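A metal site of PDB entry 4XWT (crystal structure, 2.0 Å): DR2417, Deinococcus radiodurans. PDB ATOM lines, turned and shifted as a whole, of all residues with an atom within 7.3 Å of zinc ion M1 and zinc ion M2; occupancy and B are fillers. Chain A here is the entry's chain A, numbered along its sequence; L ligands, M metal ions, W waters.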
ATOM      1  N   ILE A  30     -15.605 -12.868  -5.656  1.00  0.00           N
ATOM      2  CA  ILE A  30     -15.320 -13.621  -4.461  1.00  0.00           C
ATOM      3  C   ILE A  30     -13.979 -13.138  -3.915  1.00  0.00           C
ATOM      4  O   ILE A  30     -12.917 -13.509  -4.420  1.00  0.00           O
ATOM      5  CB  ILE A  30     -15.323 -15.113  -4.748  1.00  0.00           C
ATOM      6  CG1 ILE A  30     -16.712 -15.531  -5.222  1.00  0.00           C
ATOM      7  CG2 ILE A  30     -14.995 -15.882  -3.502  1.00  0.00           C
ATOM      8  CD1 ILE A  30     -16.842 -17.012  -5.453  1.00  0.00           C
ATOM      9  N   GLY A  31     -14.012 -12.270  -2.899  1.00  0.00           N
ATOM     10  CA  GLY A  31     -12.777 -11.659  -2.428  1.00  0.00           C
ATOM     11  C   GLY A  31     -12.890 -10.210  -1.967  1.00  0.00           C
ATOM     12  O   GLY A  31     -13.882  -9.532  -2.249  1.00  0.00           O
ATOM     13  N   ASN A  33     -13.748  -8.652   0.747  1.00  0.00           N
ATOM     14  CA  ASN A  33     -14.989  -8.242   1.384  1.00  0.00           C
ATOM     15  C   ASN A  33     -14.838  -7.046   2.332  1.00  0.00           C
ATOM     16  O   ASN A  33     -13.981  -7.026   3.223  1.00  0.00           O
ATOM     17  CB  ASN A  33     -15.593  -9.448   2.112  1.00  0.00           C
ATOM     18  CG  ASN A  33     -15.978 -10.563   1.138  1.00  0.00           C
ATOM     19  OD1 ASN A  33     -16.990 -10.468   0.439  1.00  0.00           O
ATOM     20  ND2 ASN A  33     -15.140 -11.603   1.070  1.00  0.00           N
ATOM     21  N   ASP A  47     -15.720  -6.158   7.996  1.00  0.00           N
ATOM     22  CA  ASP A  47     -14.556  -6.793   7.347  1.00  0.00           C
ATOM     23  C   ASP A  47     -13.709  -5.824   6.517  1.00  0.00           C
ATOM     24  O   ASP A  47     -14.016  -4.624   6.406  1.00  0.00           O
ATOM     25  CB  ASP A  47     -15.022  -7.997   6.499  1.00  0.00           C
ATOM     26  CG  ASP A  47     -15.556  -9.139   7.360  1.00  0.00           C
ATOM     27  OD1 ASP A  47     -15.257  -9.134   8.570  1.00  0.00           O
ATOM     28  OD2 ASP A  47     -16.273 -10.041   6.853  1.00  0.00           O
ATOM     29  N   THR A  83     -16.088 -10.643  10.849  1.00  0.00           N
ATOM     30  CA  THR A  83     -16.882 -11.857  10.903  1.00  0.00           C
ATOM     31  C   THR A  83     -16.054 -13.139  11.083  1.00  0.00           C
ATOM     32  O   THR A  83     -16.474 -14.063  11.776  1.00  0.00           O
ATOM     33  CB  THR A  83     -17.732 -12.033   9.635  1.00  0.00           C
ATOM     34  OG1 THR A  83     -16.856 -12.248   8.504  1.00  0.00           O
ATOM     35  CG2 THR A  83     -18.586 -10.800   9.382  1.00  0.00           C
ATOM     36  N   HIS A  84     -14.895 -13.206  10.411  1.00  0.00           N
ATOM     37  CA  HIS A  84     -13.973 -14.324  10.592  1.00  0.00           C
ATOM     38  C   HIS A  84     -12.589 -14.035  10.007  1.00  0.00           C
ATOM     39  O   HIS A  84     -12.378 -13.024   9.348  1.00  0.00           O
ATOM     40  CB  HIS A  84     -14.542 -15.622   9.991  1.00  0.00           C
ATOM     41  CG  HIS A  84     -14.782 -15.553   8.511  1.00  0.00           C
ATOM     42  ND1 HIS A  84     -15.586 -14.592   7.934  1.00  0.00           N
ATOM     43  CD2 HIS A  84     -14.365 -16.356   7.496  1.00  0.00           C
ATOM     44  CE1 HIS A  84     -15.646 -14.800   6.627  1.00  0.00           C
ATOM     45  NE2 HIS A  84     -14.902 -15.845   6.336  1.00  0.00           N
ATOM     46  N   GLY A  85     -11.650 -14.939  10.259  1.00  0.00           N
ATOM     47  CA  GLY A  85     -10.256 -14.662  10.010  1.00  0.00           C
ATOM     48  C   GLY A  85      -9.726 -15.081   8.635  1.00  0.00           C
ATOM     49  O   GLY A  85      -8.531 -15.172   8.470  1.00  0.00           O
ATOM     50  N   HIS A  86     -10.605 -15.326   7.665  1.00  0.00           N
ATOM     51  CA  HIS A  86     -10.118 -15.642   6.310  1.00  0.00           C
ATOM     52  C   HIS A  86      -9.492 -14.414   5.645  1.00  0.00           C
ATOM     53  O   HIS A  86      -9.826 -13.277   5.977  1.00  0.00           O
ATOM     54  CB  HIS A  86     -11.247 -16.174   5.430  1.00  0.00           C
ATOM     55  CG  HIS A  86     -11.465 -17.632   5.575  1.00  0.00           C
ATOM     56  ND1 HIS A  86     -12.678 -18.237   5.332  1.00  0.00           N
ATOM     57  CD2 HIS A  86     -10.631 -18.625   5.970  1.00  0.00           C
ATOM     58  CE1 HIS A  86     -12.569 -19.543   5.549  1.00  0.00           C
ATOM     59  NE2 HIS A  86     -11.341 -19.798   5.945  1.00  0.00           N
ATOM     60  N   GLU A  87      -8.582 -14.648   4.689  1.00  0.00           N
ATOM     61  CA  GLU A  87      -7.852 -13.532   4.101  1.00  0.00           C
ATOM     62  C   GLU A  87      -8.764 -12.583   3.336  1.00  0.00           C
ATOM     63  O   GLU A  87      -8.502 -11.387   3.280  1.00  0.00           O
ATOM     64  CB  GLU A  87      -6.735 -14.046   3.180  1.00  0.00           C
ATOM     65  CG  GLU A  87      -5.521 -14.624   3.884  1.00  0.00           C
ATOM     66  CD  GLU A  87      -4.457 -13.578   4.165  1.00  0.00           C
ATOM     67  OE1 GLU A  87      -4.762 -12.614   4.892  1.00  0.00           O
ATOM     68  OE2 GLU A  87      -3.318 -13.718   3.636  1.00  0.00           O
ATOM     69  N   ASP A  88      -9.827 -13.089   2.707  1.00  0.00           N
ATOM     70  CA  ASP A  88     -10.716 -12.156   2.022  1.00  0.00           C
ATOM     71  C   ASP A  88     -11.660 -11.390   2.977  1.00  0.00           C
ATOM     72  O   ASP A  88     -12.614 -10.767   2.516  1.00  0.00           O
ATOM     73  CB  ASP A  88     -11.553 -12.881   0.951  1.00  0.00           C
ATOM     74  CG  ASP A  88     -12.332 -14.040   1.514  1.00  0.00           C
ATOM     75  OD1 ASP A  88     -11.731 -14.827   2.277  1.00  0.00           O
ATOM     76  OD2 ASP A  88     -13.527 -14.186   1.181  1.00  0.00           O
ATOM     77  N   HIS A  89     -11.371 -11.421   4.293  1.00  0.00           N
ATOM     78  CA  HIS A  89     -12.128 -10.618   5.274  1.00  0.00           C
ATOM     79  C   HIS A  89     -11.221  -9.802   6.193  1.00  0.00           C
ATOM     80  O   HIS A  89     -11.630  -8.743   6.658  1.00  0.00           O
ATOM     81  CB  HIS A  89     -13.086 -11.515   6.077  1.00  0.00           C
ATOM     82  CG  HIS A  89     -14.044 -12.269   5.207  1.00  0.00           C
ATOM     83  ND1 HIS A  89     -15.344 -11.866   5.007  1.00  0.00           N
ATOM     84  CD2 HIS A  89     -13.856 -13.339   4.390  1.00  0.00           C
ATOM     85  CE1 HIS A  89     -15.933 -12.679   4.159  1.00  0.00           C
ATOM     86  NE2 HIS A  89     -15.052 -13.598   3.772  1.00  0.00           N
ATOM     87  N   HIS A 153     -18.563 -22.655   9.439  1.00  0.00           N
ATOM     88  CA  HIS A 153     -17.864 -22.310   8.204  1.00  0.00           C
ATOM     89  C   HIS A 153     -16.604 -23.178   8.152  1.00  0.00           C
ATOM     90  O   HIS A 153     -16.509 -24.153   8.898  1.00  0.00           O
ATOM     91  CB  HIS A 153     -17.585 -20.778   8.196  1.00  0.00           C
ATOM     92  CG  HIS A 153     -16.942 -20.267   6.948  1.00  0.00           C
ATOM     93  ND1 HIS A 153     -17.237 -20.759   5.688  1.00  0.00           N
ATOM     94  CD2 HIS A 153     -16.020 -19.298   6.757  1.00  0.00           C
ATOM     95  CE1 HIS A 153     -16.518 -20.123   4.783  1.00  0.00           C
ATOM     96  NE2 HIS A 153     -15.764 -19.229   5.404  1.00  0.00           N
ATOM     97  N   SER A 154     -15.646 -22.867   7.287  1.00  0.00           N
ATOM     98  CA  SER A 154     -14.426 -23.673   7.151  1.00  0.00           C
ATOM     99  C   SER A 154     -13.299 -23.175   8.059  1.00  0.00           C
ATOM    100  O   SER A 154     -12.150 -23.652   7.987  1.00  0.00           O
ATOM    101  CB  SER A 154     -13.957 -23.668   5.696  1.00  0.00           C
ATOM    102  OG  SER A 154     -13.782 -22.308   5.327  1.00  0.00           O
ATOM    103  N   ILE A 155     -13.622 -22.191   8.907  1.00  0.00           N
ATOM    104  CA  ILE A 155     -12.706 -21.723   9.950  1.00  0.00           C
ATOM    105  C   ILE A 155     -13.518 -21.515  11.246  1.00  0.00           C
ATOM    106  O   ILE A 155     -14.684 -21.137  11.191  1.00  0.00           O
ATOM    107  CB  ILE A 155     -11.954 -20.415   9.536  1.00  0.00           C
ATOM    108  CG1 ILE A 155     -10.717 -20.187  10.417  1.00  0.00           C
ATOM    109  CG2 ILE A 155     -12.900 -19.196   9.550  1.00  0.00           C
ATOM    110  CD1 ILE A 155      -9.859 -18.937  10.077  1.00  0.00           C
ATOM    111  N   ASN A 158     -16.457 -18.108  13.513  1.00  0.00           N
ATOM    112  CA  ASN A 158     -17.027 -17.465  12.350  1.00  0.00           C
ATOM    113  C   ASN A 158     -18.405 -17.013  12.732  1.00  0.00           C
ATOM    114  O   ASN A 158     -19.174 -17.799  13.289  1.00  0.00           O
ATOM    115  CB  ASN A 158     -17.042 -18.438  11.181  1.00  0.00           C
ATOM    116  CG  ASN A 158     -17.790 -17.925   9.993  1.00  0.00           C
ATOM    117  OD1 ASN A 158     -17.250 -17.178   9.174  1.00  0.00           O
ATOM    118  ND2 ASN A 158     -19.034 -18.345   9.858  1.00  0.00           N
ATOM    119  N   GLY A 174     -22.857 -13.726   7.179  1.00  0.00           N
ATOM    120  CA  GLY A 174     -21.437 -13.901   7.049  1.00  0.00           C
ATOM    121  C   GLY A 174     -21.201 -15.023   6.042  1.00  0.00           C
ATOM    122  O   GLY A 174     -22.101 -15.381   5.279  1.00  0.00           O
ATOM    123  N   ASP A 175     -19.983 -15.558   6.014  1.00  0.00           N
ATOM    124  CA  ASP A 175     -19.705 -16.805   5.303  1.00  0.00           C
ATOM    125  C   ASP A 175     -20.317 -17.968   6.054  1.00  0.00           C
ATOM    126  O   ASP A 175     -20.165 -18.042   7.279  1.00  0.00           O
ATOM    127  CB  ASP A 175     -18.193 -17.040   5.178  1.00  0.00           C
ATOM    128  CG  ASP A 175     -17.513 -16.118   4.184  1.00  0.00           C
ATOM    129  OD1 ASP A 175     -18.008 -14.968   3.986  1.00  0.00           O
ATOM    130  OD2 ASP A 175     -16.471 -16.566   3.632  1.00  0.00           O
ATOM    131  N   PHE A 176     -20.990 -18.887   5.362  1.00  0.00           N
ATOM    132  CA  PHE A 176     -21.527 -20.051   6.062  1.00  0.00           C
ATOM    133  C   PHE A 176     -21.826 -21.276   5.218  1.00  0.00           C
ATOM    134  O   PHE A 176     -22.085 -21.190   4.019  1.00  0.00           O
ATOM    135  CB  PHE A 176     -22.823 -19.683   6.774  1.00  0.00           C
ATOM    136  CG  PHE A 176     -24.043 -19.697   5.898  1.00  0.00           C
ATOM    137  CD1 PHE A 176     -24.320 -18.619   5.071  1.00  0.00           C
ATOM    138  CD2 PHE A 176     -24.944 -20.752   5.941  1.00  0.00           C
ATOM    139  CE1 PHE A 176     -25.460 -18.603   4.289  1.00  0.00           C
ATOM    140  CE2 PHE A 176     -26.110 -20.755   5.151  1.00  0.00           C
ATOM    141  CZ  PHE A 176     -26.363 -19.673   4.317  1.00  0.00           C
ATOM    142  N   ASP A 209     -24.501 -15.383   1.837  1.00  0.00           N
ATOM    143  CA  ASP A 209     -23.334 -15.914   1.161  1.00  0.00           C
ATOM    144  C   ASP A 209     -23.703 -16.690  -0.106  1.00  0.00           C
ATOM    145  O   ASP A 209     -24.355 -17.722  -0.015  1.00  0.00           O
ATOM    146  CB  ASP A 209     -22.571 -16.805   2.147  1.00  0.00           C
ATOM    147  CG  ASP A 209     -21.377 -17.518   1.531  1.00  0.00           C
ATOM    148  OD1 ASP A 209     -21.014 -17.267   0.364  1.00  0.00           O
ATOM    149  OD2 ASP A 209     -20.773 -18.332   2.251  1.00  0.00           O
ATOM    150  N   THR A 211     -21.612 -17.993  -2.587  1.00  0.00           N
ATOM    151  CA  THR A 211     -20.485 -18.697  -3.200  1.00  0.00           C
ATOM    152  C   THR A 211     -20.933 -19.929  -3.974  1.00  0.00           C
ATOM    153  O   THR A 211     -20.551 -20.136  -5.134  1.00  0.00           O
ATOM    154  CB  THR A 211     -19.450 -19.141  -2.149  1.00  0.00           C
ATOM    155  OG1 THR A 211     -18.978 -18.000  -1.417  1.00  0.00           O
ATOM    156  CG2 THR A 211     -18.269 -19.829  -2.826  1.00  0.00           C
ATOM    157  N   GLY A 380     -16.569 -24.733   2.292  1.00  0.00           N
ATOM    158  CA  GLY A 380     -16.962 -24.009   3.485  1.00  0.00           C
ATOM    159  C   GLY A 380     -18.279 -23.267   3.324  1.00  0.00           C
ATOM    160  O   GLY A 380     -18.725 -22.612   4.255  1.00  0.00           O
ATOM    161  N   HIS A 381     -18.906 -23.421   2.165  1.00  0.00           N
ATOM    162  CA  HIS A 381     -20.059 -22.600   1.823  1.00  0.00           C
ATOM    163  C   HIS A 381     -21.312 -23.416   1.547  1.00  0.00           C
ATOM    164  O   HIS A 381     -21.266 -24.492   0.949  1.00  0.00           O
ATOM    165  CB  HIS A 381     -19.738 -21.721   0.608  1.00  0.00           C
ATOM    166  CG  HIS A 381     -18.616 -20.769   0.857  1.00  0.00           C
ATOM    167  ND1 HIS A 381     -18.821 -19.458   1.260  1.00  0.00           N
ATOM    168  CD2 HIS A 381     -17.272 -20.915   0.775  1.00  0.00           C
ATOM    169  CE1 HIS A 381     -17.660 -18.855   1.401  1.00  0.00           C
ATOM    170  NE2 HIS A 381     -16.694 -19.720   1.110  1.00  0.00           N
ATOM    171  N   TRP A 402     -24.838 -11.785  -1.821  1.00  0.00           N
ATOM    172  CA  TRP A 402     -23.515 -11.210  -1.607  1.00  0.00           C
ATOM    173  C   TRP A 402     -22.431 -12.313  -1.644  1.00  0.00           C
ATOM    174  O   TRP A 402     -22.778 -13.493  -1.752  1.00  0.00           O
ATOM    175  CB  TRP A 402     -23.551 -10.430  -0.266  1.00  0.00           C
ATOM    176  CG  TRP A 402     -22.268 -10.288   0.451  1.00  0.00           C
ATOM    177  CD1 TRP A 402     -21.369  -9.291   0.287  1.00  0.00           C
ATOM    178  CD2 TRP A 402     -21.728 -11.188   1.435  1.00  0.00           C
ATOM    179  NE1 TRP A 402     -20.291  -9.504   1.115  1.00  0.00           N
ATOM    180  CE2 TRP A 402     -20.482 -10.667   1.816  1.00  0.00           C
ATOM    181  CE3 TRP A 402     -22.165 -12.383   2.004  1.00  0.00           C
ATOM    182  CZ2 TRP A 402     -19.662 -11.296   2.759  1.00  0.00           C
ATOM    183  CZ3 TRP A 402     -21.359 -13.014   2.944  1.00  0.00           C
ATOM    184  CH2 TRP A 402     -20.125 -12.453   3.326  1.00  0.00           C
ATOM    185  N   HIS A 403     -21.137 -11.963  -1.590  1.00  0.00           N
ATOM    186  CA  HIS A 403     -20.003 -12.914  -1.620  1.00  0.00           C
ATOM    187  C   HIS A 403     -20.091 -13.853  -2.834  1.00  0.00           C
ATOM    188  O   HIS A 403     -20.069 -15.068  -2.704  1.00  0.00           O
ATOM    189  CB  HIS A 403     -19.933 -13.754  -0.310  1.00  0.00           C
ATOM    190  CG  HIS A 403     -18.561 -14.271   0.062  1.00  0.00           C
ATOM    191  ND1 HIS A 403     -17.931 -15.307  -0.588  1.00  0.00           N
ATOM    192  CD2 HIS A 403     -17.731 -13.909   1.079  1.00  0.00           C
ATOM    193  CE1 HIS A 403     -16.770 -15.561   0.007  1.00  0.00           C
ATOM    194  NE2 HIS A 403     -16.627 -14.724   1.022  1.00  0.00           N
HETATM  195  N1  LIG L   1     -11.171 -20.184  -0.634  1.00  0.00           N
HETATM  196  C1  LIG L   1     -10.111 -19.295  -0.369  1.00  0.00           C
HETATM  197  N2  LIG L   1      -9.449 -19.360   0.789  1.00  0.00           N
HETATM  198  C2  LIG L   1      -9.780 -20.258   1.717  1.00  0.00           C
HETATM  199  C3  LIG L   1     -10.832 -21.146   1.487  1.00  0.00           C
HETATM  200  C4  LIG L   1     -11.516 -21.083   0.292  1.00  0.00           C
HETATM  201  O1  LIG L   1      -9.791 -18.439  -1.222  1.00  0.00           O
HETATM  202  O2  LIG L   1      -9.152 -20.300   2.777  1.00  0.00           O
HETATM  203  C5  LIG L   1     -11.907 -20.103  -1.907  1.00  0.00           C
HETATM  204  C6  LIG L   1     -12.042 -21.470  -2.555  1.00  0.00           C
HETATM  205  O3  LIG L   1     -11.155 -21.592  -3.671  1.00  0.00           O
HETATM  206  C7  LIG L   1     -13.480 -21.536  -3.016  1.00  0.00           C
HETATM  207  C8  LIG L   1     -14.209 -20.570  -2.118  1.00  0.00           C
HETATM  208  O4  LIG L   1     -13.597 -21.056  -4.358  1.00  0.00           O
HETATM  209  O5  LIG L   1     -13.233 -19.635  -1.657  1.00  0.00           O
HETATM  210  C9  LIG L   1     -14.798 -21.306  -0.931  1.00  0.00           C
HETATM  211  O6  LIG L   1     -13.844 -22.248  -0.431  1.00  0.00           O
HETATM  212  P1  LIG L   1     -14.222 -23.191   0.813  1.00  0.00           P
HETATM  213  O7  LIG L   1     -15.436 -23.871   0.266  1.00  0.00           O
HETATM  214  O8  LIG L   1     -13.027 -24.083   1.040  1.00  0.00           O
HETATM  215  O9  LIG L   1     -14.445 -22.236   1.948  1.00  0.00           O
HETATM  216 ZN    ZN M   1     -15.207 -15.202   2.428  1.00  0.00          ZN
HETATM  217 ZN    ZN M   2     -14.498 -17.497   4.659  1.00  0.00          ZN
HETATM  218  O   HOH W   1     -13.991 -18.492   1.731  1.00  0.00           O
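A ring nitrogen (ND1) of His 84 sits at hydrogen-bond distance from the side-chain hydroxyl (OG1) of Thr 83. ND1 of His 153 sits at hydrogen-bond distance from O of Gly 380, 2.8 Å away. The backbone carbonyl oxygen (O) of Asp 175 is in hydrogen-bond range of the side-chain amide nitrogen (ND2) of Asn 158 (2.8 Å). A ring nitrogen (ND1) of His 89 lies within hydrogen-bond range of the side-chain carboxylate of Asp 47. The side-chain hydroxyl of Thr 211 lies within hydrogen-bond range of a ring nitrogen (ND1) of His 403 (3.0 Å). NE2 of His 403 lies close to ND2 of Asn 33, at 3.5 Å. The side-chain amide nitrogen (ND2) of Asn 33 sits close to a ring nitrogen (NE2) of His 89. OD1 of Asn 158 lies close to ND1 of His 84.
The nearest printed residue that does not touch zinc ion M2 is His 89 (4.04 Å).
Zinc ion M2 is bound by a ring nitrogen (ND1) of His 86 (2.1 Å), a ring nitrogen (NE2) of His 153 (2.3 Å), a ring nitrogen (NE2) of His 84 (2.4 Å) and the side-chain carboxylate of Asp 175 (2.4 Å). Zinc ion M2 has four donor atoms within binding distance.
Zinc ion M1 is bound by a ring nitrogen (NE2) of His 403, a ring nitrogen (NE2) of His 89, the side-chain carboxylate (OD2) of Asp 175 and the side-chain carboxylate (OD2) of Asp 88.
Residues that only touch zinc ion M1: Asn 33. Six residues have an atom within 4 Å of zinc ion M1: Asn 33, His 84, Asp 88, His 89, Asp 175 and His 403. The nearest printed residue that does not touch zinc ion M1 is His 381 (4.5 Å).
The backbone NH of Gly 380 sits at hydrogen-bond distance from an oxygen (O7) of the ligand (2.5 Å). O9 of the ligand sits close to NE2 of His 381, 3.5 Å away. O9 of the ligand is in hydrogen-bond range of OG of Ser 154 (3.4 Å).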
